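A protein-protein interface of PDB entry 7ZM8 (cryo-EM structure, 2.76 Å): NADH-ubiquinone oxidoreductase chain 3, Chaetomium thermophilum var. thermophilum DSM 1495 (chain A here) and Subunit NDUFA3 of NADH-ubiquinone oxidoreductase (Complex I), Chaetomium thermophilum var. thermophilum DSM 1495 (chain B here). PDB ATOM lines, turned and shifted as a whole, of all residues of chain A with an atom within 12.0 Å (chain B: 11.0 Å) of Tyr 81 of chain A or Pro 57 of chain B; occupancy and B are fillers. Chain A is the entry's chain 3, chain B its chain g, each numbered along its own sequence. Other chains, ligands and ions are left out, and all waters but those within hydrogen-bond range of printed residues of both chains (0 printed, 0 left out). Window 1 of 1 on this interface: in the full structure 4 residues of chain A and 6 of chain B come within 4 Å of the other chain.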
ATOM      1  N   LEU A  73     -19.959 -31.226 -30.842  1.00  0.00           N
ATOM      2  CA  LEU A  73     -20.885 -31.532 -29.762  1.00  0.00           C
ATOM      3  C   LEU A  73     -20.211 -32.157 -28.549  1.00  0.00           C
ATOM      4  O   LEU A  73     -20.780 -32.116 -27.455  1.00  0.00           O
ATOM      5  CB  LEU A  73     -21.978 -32.472 -30.269  1.00  0.00           C
ATOM      6  CG  LEU A  73     -23.125 -31.832 -31.038  1.00  0.00           C
ATOM      7  CD1 LEU A  73     -24.052 -32.908 -31.536  1.00  0.00           C
ATOM      8  CD2 LEU A  73     -23.861 -30.842 -30.151  1.00  0.00           C
ATOM      9  N   TYR A  74     -19.025 -32.733 -28.716  1.00  0.00           N
ATOM     10  CA  TYR A  74     -18.324 -33.329 -27.583  1.00  0.00           C
ATOM     11  C   TYR A  74     -18.024 -32.345 -26.457  1.00  0.00           C
ATOM     12  O   TYR A  74     -18.099 -32.760 -25.288  1.00  0.00           O
ATOM     13  CB  TYR A  74     -17.041 -34.014 -28.065  1.00  0.00           C
ATOM     14  CG  TYR A  74     -17.240 -35.474 -28.383  1.00  0.00           C
ATOM     15  CD1 TYR A  74     -17.680 -35.873 -29.633  1.00  0.00           C
ATOM     16  CD2 TYR A  74     -17.018 -36.451 -27.427  1.00  0.00           C
ATOM     17  CE1 TYR A  74     -17.878 -37.198 -29.929  1.00  0.00           C
ATOM     18  CE2 TYR A  74     -17.216 -37.785 -27.713  1.00  0.00           C
ATOM     19  CZ  TYR A  74     -17.647 -38.151 -28.970  1.00  0.00           C
ATOM     20  OH  TYR A  74     -17.846 -39.473 -29.277  1.00  0.00           O
ATOM     21  N   PRO A  75     -17.642 -31.087 -26.709  1.00  0.00           N
ATOM     22  CA  PRO A  75     -17.490 -30.153 -25.584  1.00  0.00           C
ATOM     23  C   PRO A  75     -18.763 -29.938 -24.791  1.00  0.00           C
ATOM     24  O   PRO A  75     -18.688 -29.692 -23.584  1.00  0.00           O
ATOM     25  CB  PRO A  75     -17.021 -28.865 -26.270  1.00  0.00           C
ATOM     26  CG  PRO A  75     -16.395 -29.313 -27.508  1.00  0.00           C
ATOM     27  CD  PRO A  75     -17.193 -30.473 -27.970  1.00  0.00           C
ATOM     28  N   PHE A  76     -19.931 -30.017 -25.429  1.00  0.00           N
ATOM     29  CA  PHE A  76     -21.181 -29.834 -24.703  1.00  0.00           C
ATOM     30  C   PHE A  76     -21.396 -30.938 -23.682  1.00  0.00           C
ATOM     31  O   PHE A  76     -21.883 -30.682 -22.577  1.00  0.00           O
ATOM     32  CB  PHE A  76     -22.357 -29.779 -25.678  1.00  0.00           C
ATOM     33  CG  PHE A  76     -23.687 -29.658 -25.006  1.00  0.00           C
ATOM     34  CD1 PHE A  76     -24.140 -28.436 -24.565  1.00  0.00           C
ATOM     35  CD2 PHE A  76     -24.478 -30.775 -24.804  1.00  0.00           C
ATOM     36  CE1 PHE A  76     -25.353 -28.329 -23.936  1.00  0.00           C
ATOM     37  CE2 PHE A  76     -25.692 -30.669 -24.176  1.00  0.00           C
ATOM     38  CZ  PHE A  76     -26.132 -29.445 -23.744  1.00  0.00           C
ATOM     39  N   ALA A  77     -21.050 -32.175 -24.038  1.00  0.00           N
ATOM     40  CA  ALA A  77     -21.290 -33.308 -23.155  1.00  0.00           C
ATOM     41  C   ALA A  77     -20.450 -33.252 -21.888  1.00  0.00           C
ATOM     42  O   ALA A  77     -20.897 -33.736 -20.846  1.00  0.00           O
ATOM     43  CB  ALA A  77     -21.025 -34.612 -23.897  1.00  0.00           C
ATOM     44  N   VAL A  78     -19.251 -32.675 -21.947  1.00  0.00           N
ATOM     45  CA  VAL A  78     -18.407 -32.540 -20.770  1.00  0.00           C
ATOM     46  C   VAL A  78     -18.514 -31.152 -20.153  1.00  0.00           C
ATOM     47  O   VAL A  78     -17.650 -30.759 -19.369  1.00  0.00           O
ATOM     48  CB  VAL A  78     -16.943 -32.894 -21.088  1.00  0.00           C
ATOM     49  CG1 VAL A  78     -16.818 -34.357 -21.425  1.00  0.00           C
ATOM     50  CG2 VAL A  78     -16.424 -32.056 -22.236  1.00  0.00           C
ATOM     51  N   SER A  79     -19.542 -30.387 -20.511  1.00  0.00           N
ATOM     52  CA  SER A  79     -19.813 -29.119 -19.852  1.00  0.00           C
ATOM     53  C   SER A  79     -21.310 -28.888 -19.683  1.00  0.00           C
ATOM     54  O   SER A  79     -21.765 -27.741 -19.678  1.00  0.00           O
ATOM     55  CB  SER A  79     -19.172 -27.958 -20.612  1.00  0.00           C
ATOM     56  OG  SER A  79     -19.754 -27.782 -21.886  1.00  0.00           O
ATOM     57  N   GLU A  80     -22.107 -29.929 -19.481  1.00  0.00           N
ATOM     58  CA  GLU A  80     -23.597 -29.796 -19.401  1.00  0.00           C
ATOM     59  C   GLU A  80     -24.084 -29.143 -18.109  1.00  0.00           C
ATOM     60  O   GLU A  80     -25.134 -28.515 -18.152  1.00  0.00           O
ATOM     61  CB  GLU A  80     -24.293 -31.149 -19.538  1.00  0.00           C
ATOM     62  CG  GLU A  80     -24.500 -31.600 -20.965  1.00  0.00           C
ATOM     63  CD  GLU A  80     -24.733 -33.094 -21.068  1.00  0.00           C
ATOM     64  OE1 GLU A  80     -25.414 -33.527 -22.016  1.00  0.00           O
ATOM     65  OE2 GLU A  80     -24.232 -33.816 -20.196  1.00  0.00           O
ATOM     66  N   TYR A  81     -23.387 -29.317 -16.999  1.00  0.00           N
ATOM     67  CA  TYR A  81     -23.851 -28.778 -15.701  1.00  0.00           C
ATOM     68  C   TYR A  81     -23.887 -27.251 -15.754  1.00  0.00           C
ATOM     69  O   TYR A  81     -24.750 -26.631 -15.133  1.00  0.00           O
ATOM     70  CB  TYR A  81     -23.048 -29.360 -14.539  1.00  0.00           C
ATOM     71  CG  TYR A  81     -23.586 -29.024 -13.174  1.00  0.00           C
ATOM     72  CD1 TYR A  81     -24.566 -29.810 -12.595  1.00  0.00           C
ATOM     73  CD2 TYR A  81     -23.124 -27.925 -12.468  1.00  0.00           C
ATOM     74  CE1 TYR A  81     -25.070 -29.516 -11.343  1.00  0.00           C
ATOM     75  CE2 TYR A  81     -23.628 -27.614 -11.217  1.00  0.00           C
ATOM     76  CZ  TYR A  81     -24.601 -28.416 -10.653  1.00  0.00           C
ATOM     77  OH  TYR A  81     -25.114 -28.140  -9.424  1.00  0.00           O
ATOM     78  N   VAL A  82     -22.938 -26.661 -16.485  1.00  0.00           N
ATOM     79  CA  VAL A  82     -22.865 -25.176 -16.621  1.00  0.00           C
ATOM     80  C   VAL A  82     -23.707 -24.755 -17.828  1.00  0.00           C
ATOM     81  O   VAL A  82     -24.513 -23.832 -17.685  1.00  0.00           O
ATOM     82  CB  VAL A  82     -21.401 -24.700 -16.724  1.00  0.00           C
ATOM     83  CG1 VAL A  82     -21.274 -23.319 -17.347  1.00  0.00           C
ATOM     84  CG2 VAL A  82     -20.699 -24.753 -15.378  1.00  0.00           C
ATOM     85  N   ASN A  83     -23.579 -25.419 -18.970  1.00  0.00           N
ATOM     86  CA  ASN A  83     -24.354 -24.951 -20.141  1.00  0.00           C
ATOM     87  C   ASN A  83     -25.806 -24.852 -19.688  1.00  0.00           C
ATOM     88  O   ASN A  83     -26.423 -23.799 -19.939  1.00  0.00           O
ATOM     89  CB  ASN A  83     -24.126 -25.843 -21.363  1.00  0.00           C
ATOM     90  CG  ASN A  83     -22.866 -25.497 -22.125  1.00  0.00           C
ATOM     91  OD1 ASN A  83     -22.188 -26.380 -22.644  1.00  0.00           O
ATOM     92  ND2 ASN A  83     -22.538 -24.218 -22.192  1.00  0.00           N
ATOM     93  N   SER A  84     -26.318 -25.902 -19.039  1.00  0.00           N
ATOM     94  CA  SER A  84     -27.699 -25.923 -18.493  1.00  0.00           C
ATOM     95  C   SER A  84     -28.751 -25.688 -19.574  1.00  0.00           C
ATOM     96  O   SER A  84     -28.562 -26.197 -20.683  1.00  0.00           O
ATOM     97  CB  SER A  84     -27.849 -24.978 -17.331  1.00  0.00           C
ATOM     98  OG  SER A  84     -29.006 -25.295 -16.572  1.00  0.00           O
ATOM     99  N   ALA A  85     -29.793 -24.918 -19.267  1.00  0.00           N
ATOM    100  CA  ALA A  85     -30.930 -24.736 -20.196  1.00  0.00           C
ATOM    101  C   ALA A  85     -30.553 -23.833 -21.368  1.00  0.00           C
ATOM    102  O   ALA A  85     -30.963 -24.147 -22.494  1.00  0.00           O
ATOM    103  CB  ALA A  85     -32.079 -24.166 -19.418  1.00  0.00           C
ATOM    104  N   TYR A  86     -29.853 -22.729 -21.103  1.00  0.00           N
ATOM    105  CA  TYR A  86     -29.407 -21.829 -22.196  1.00  0.00           C
ATOM    106  C   TYR A  86     -28.481 -22.581 -23.152  1.00  0.00           C
ATOM    107  O   TYR A  86     -28.645 -22.442 -24.376  1.00  0.00           O
ATOM    108  CB  TYR A  86     -28.784 -20.557 -21.619  1.00  0.00           C
ATOM    109  CG  TYR A  86     -28.816 -19.368 -22.545  1.00  0.00           C
ATOM    110  CD1 TYR A  86     -29.998 -18.691 -22.795  1.00  0.00           C
ATOM    111  CD2 TYR A  86     -27.665 -18.915 -23.167  1.00  0.00           C
ATOM    112  CE1 TYR A  86     -30.039 -17.601 -23.646  1.00  0.00           C
ATOM    113  CE2 TYR A  86     -27.688 -17.824 -24.019  1.00  0.00           C
ATOM    114  CZ  TYR A  86     -28.879 -17.165 -24.258  1.00  0.00           C
ATOM    115  OH  TYR A  86     -28.910 -16.088 -25.092  1.00  0.00           O
ATOM    116  N   GLY A  87     -27.539 -23.352 -22.606  1.00  0.00           N
ATOM    117  CA  GLY A  87     -26.624 -24.147 -23.443  1.00  0.00           C
ATOM    118  C   GLY A  87     -27.372 -25.221 -24.199  1.00  0.00           C
ATOM    119  O   GLY A  87     -27.055 -25.432 -25.377  1.00  0.00           O
ATOM    120  N   LEU A  88     -28.323 -25.883 -23.533  1.00  0.00           N
ATOM    121  CA  LEU A  88     -29.145 -26.919 -24.202  1.00  0.00           C
ATOM    122  C   LEU A  88     -29.809 -26.271 -25.413  1.00  0.00           C
ATOM    123  O   LEU A  88     -29.700 -26.837 -26.509  1.00  0.00           O
ATOM    124  CB  LEU A  88     -30.192 -27.457 -23.225  1.00  0.00           C
ATOM    125  CG  LEU A  88     -31.032 -28.629 -23.725  1.00  0.00           C
ATOM    126  CD1 LEU A  88     -30.146 -29.781 -24.168  1.00  0.00           C
ATOM    127  CD2 LEU A  88     -32.006 -29.088 -22.654  1.00  0.00           C
ATOM    128  N   ALA A  89     -30.444 -25.113 -25.219  1.00  0.00           N
ATOM    129  CA  ALA A  89     -31.170 -24.502 -26.347  1.00  0.00           C
ATOM    130  C   ALA A  89     -30.234 -24.313 -27.533  1.00  0.00           C
ATOM    131  O   ALA A  89     -30.619 -24.696 -28.633  1.00  0.00           O
ATOM    132  CB  ALA A  89     -31.665 -23.168 -25.903  1.00  0.00           C
ATOM    133  N   ALA A  91     -27.359 -25.699 -28.269  1.00  0.00           N
ATOM    134  CA  ALA A  91     -26.928 -26.984 -28.806  1.00  0.00           C
ATOM    135  C   ALA A  91     -28.041 -27.664 -29.585  1.00  0.00           C
ATOM    136  O   ALA A  91     -27.773 -28.347 -30.577  1.00  0.00           O
ATOM    137  CB  ALA A  91     -26.437 -27.881 -27.674  1.00  0.00           C
ATOM    138  N   VAL B  53     -38.060 -30.470  -6.451  1.00  0.00           N
ATOM    139  CA  VAL B  53     -37.400 -29.165  -6.753  1.00  0.00           C
ATOM    140  C   VAL B  53     -36.046 -29.379  -7.416  1.00  0.00           C
ATOM    141  O   VAL B  53     -35.487 -30.470  -7.271  1.00  0.00           O
ATOM    142  CB  VAL B  53     -37.287 -28.275  -5.502  1.00  0.00           C
ATOM    143  CG1 VAL B  53     -38.643 -28.051  -4.851  1.00  0.00           C
ATOM    144  CG2 VAL B  53     -36.292 -28.821  -4.491  1.00  0.00           C
ATOM    145  N   ASP B  54     -35.580 -28.391  -8.173  1.00  0.00           N
ATOM    146  CA  ASP B  54     -34.213 -28.468  -8.743  1.00  0.00           C
ATOM    147  C   ASP B  54     -33.205 -28.237  -7.623  1.00  0.00           C
ATOM    148  O   ASP B  54     -33.513 -27.466  -6.699  1.00  0.00           O
ATOM    149  CB  ASP B  54     -33.971 -27.421  -9.828  1.00  0.00           C
ATOM    150  CG  ASP B  54     -34.773 -27.663 -11.096  1.00  0.00           C
ATOM    151  OD1 ASP B  54     -34.404 -27.088 -12.138  1.00  0.00           O
ATOM    152  OD2 ASP B  54     -35.762 -28.418 -11.031  1.00  0.00           O
ATOM    153  N   ALA B  55     -32.055 -28.890  -7.706  1.00  0.00           N
ATOM    154  CA  ALA B  55     -30.982 -28.661  -6.726  1.00  0.00           C
ATOM    155  C   ALA B  55     -30.402 -27.272  -6.974  1.00  0.00           C
ATOM    156  O   ALA B  55     -30.416 -26.839  -8.136  1.00  0.00           O
ATOM    157  CB  ALA B  55     -29.950 -29.730  -6.931  1.00  0.00           C
ATOM    158  N   ALA B  56     -29.916 -26.592  -5.934  1.00  0.00           N
ATOM    159  CA  ALA B  56     -29.230 -25.298  -6.150  1.00  0.00           C
ATOM    160  C   ALA B  56     -27.942 -25.600  -6.905  1.00  0.00           C
ATOM    161  O   ALA B  56     -27.452 -26.732  -6.779  1.00  0.00           O
ATOM    162  CB  ALA B  56     -28.941 -24.641  -4.828  1.00  0.00           C
ATOM    163  N   PRO B  57     -27.358 -24.663  -7.681  1.00  0.00           N
ATOM    164  CA  PRO B  57     -26.089 -24.954  -8.331  1.00  0.00           C
ATOM    165  C   PRO B  57     -25.010 -25.195  -7.262  1.00  0.00           C
ATOM    166  O   PRO B  57     -25.059 -24.589  -6.212  1.00  0.00           O
ATOM    167  CB  PRO B  57     -25.870 -23.732  -9.228  1.00  0.00           C
ATOM    168  CG  PRO B  57     -26.676 -22.634  -8.571  1.00  0.00           C
ATOM    169  CD  PRO B  57     -27.882 -23.334  -7.984  1.00  0.00           C
ATOM    170  N   ILE B  58     -24.093 -26.122  -7.532  1.00  0.00           N
ATOM    171  CA  ILE B  58     -22.992 -26.393  -6.566  1.00  0.00           C
ATOM    172  C   ILE B  58     -21.960 -25.255  -6.651  1.00  0.00           C
ATOM    173  O   ILE B  58     -21.899 -24.628  -7.724  1.00  0.00           O
ATOM    174  CB  ILE B  58     -22.359 -27.787  -6.758  1.00  0.00           C
ATOM    175  CG1 ILE B  58     -21.481 -27.864  -8.010  1.00  0.00           C
ATOM    176  CG2 ILE B  58     -23.417 -28.878  -6.724  1.00  0.00           C
ATOM    177  CD1 ILE B  58     -20.351 -28.859  -7.899  1.00  0.00           C
ATOM    178  N   PRO B  59     -21.167 -24.918  -5.597  1.00  0.00           N
ATOM    179  CA  PRO B  59     -20.153 -23.872  -5.756  1.00  0.00           C
ATOM    180  C   PRO B  59     -18.964 -24.204  -6.682  1.00  0.00           C
ATOM    181  O   PRO B  59     -18.400 -25.247  -6.555  1.00  0.00           O
ATOM    182  CB  PRO B  59     -19.739 -23.629  -4.306  1.00  0.00           C
ATOM    183  CG  PRO B  59     -19.987 -24.938  -3.601  1.00  0.00           C
ATOM    184  CD  PRO B  59     -21.231 -25.489  -4.253  1.00  0.00           C
ATOM    185  N   LEU B  60     -18.599 -23.290  -7.580  1.00  0.00           N
ATOM    186  CA  LEU B  60     -17.493 -23.522  -8.548  1.00  0.00           C
ATOM    187  C   LEU B  60     -16.498 -22.373  -8.425  1.00  0.00           C
ATOM    188  O   LEU B  60     -15.552 -22.354  -9.206  1.00  0.00           O
ATOM    189  CB  LEU B  60     -18.051 -23.638  -9.966  1.00  0.00           C
ATOM    190  CG  LEU B  60     -18.856 -24.902 -10.261  1.00  0.00           C
ATOM    191  CD1 LEU B  60     -19.476 -24.837 -11.646  1.00  0.00           C
ATOM    192  CD2 LEU B  60     -17.991 -26.145 -10.125  1.00  0.00           C
ATOM    193  N   THR B  61     -16.722 -21.460  -7.486  1.00  0.00           N
ATOM    194  CA  THR B  61     -15.796 -20.349  -7.174  1.00  0.00           C
ATOM    195  C   THR B  61     -15.892 -20.216  -5.659  1.00  0.00           C
ATOM    196  O   THR B  61     -16.906 -20.676  -5.121  1.00  0.00           O
ATOM    197  CB  THR B  61     -16.172 -19.065  -7.930  1.00  0.00           C
ATOM    198  OG1 THR B  61     -15.065 -18.170  -7.968  1.00  0.00           O
ATOM    199  CG2 THR B  61     -17.385 -18.362  -7.363  1.00  0.00           C
ATOM    200  N   PRO B  63     -17.148 -18.902  -2.348  1.00  0.00           N
ATOM    201  CA  PRO B  63     -18.383 -18.163  -2.148  1.00  0.00           C
ATOM    202  C   PRO B  63     -18.165 -16.908  -1.304  1.00  0.00           C
ATOM    203  O   PRO B  63     -18.350 -16.970  -0.109  1.00  0.00           O
ATOM    204  CB  PRO B  63     -19.210 -19.169  -1.363  1.00  0.00           C
ATOM    205  CG  PRO B  63     -18.206 -19.959  -0.563  1.00  0.00           C
ATOM    206  CD  PRO B  63     -16.990 -20.035  -1.449  1.00  0.00           C
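N of Ile 58 of chain B lies within hydrogen-bond range of OH of Tyr 81 of chain A.
Hydrophobic or aromatic side chains of chain A within 4 Å of the printed part of chain B: Tyr 81 and Val 82.
Among the printed residues, 4 pairs touch across the chains.
Among the printed residues, no Asp or Glu carboxylate lies within 4 Å of a Lys or Arg side-chain nitrogen of the other chain.
Pro 75 of chain A touches none of the printed residues of chain B.
No residue of chain B comes within 4 Å of Ser 79 of chain A.
No residue of chain B comes within 4 Å of Glu 80 of chain A.
Of chain B, only Ala 56, Pro 57 and Ile 58 come within 4 Å of Tyr 81 of chain A.
Of chain B, only Leu 60 comes within 4 Å of Val 82 of chain A.
Ser 84 of chain A touches none of the printed residues of chain B.
Val 53 of chain B touches none of the printed residues of chain A.
Ala 55 of chain B touches none of the printed residues of chain A.
Of the printed residues of chain A, Ala 56 of chain B touches Tyr 81.
Pro 57 of chain B touches just one residue of chain A: Tyr 81 (3.5 Å).
Pro 59 of chain B touches none of the printed residues of chain A.
Of the printed residues of chain A, Leu 60 of chain B touches Val 82.
The nearest residue of chain A that does not touch Pro 57 of chain B is Val 82 of chain A (8.1 Å).
The nearest printed residue of chain A that does not touch Leu 60 of chain B is Tyr 81 of chain A (4.8 Å).
Tyr 81 of chain A touches Ala 56 of chain B (OH to O, 3.8 Å).
Tyr 81 of chain A touches Pro 57 of chain B (OH to CA, 3.5 Å).
Val 82 of chain A touches Leu 60 of chain B.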
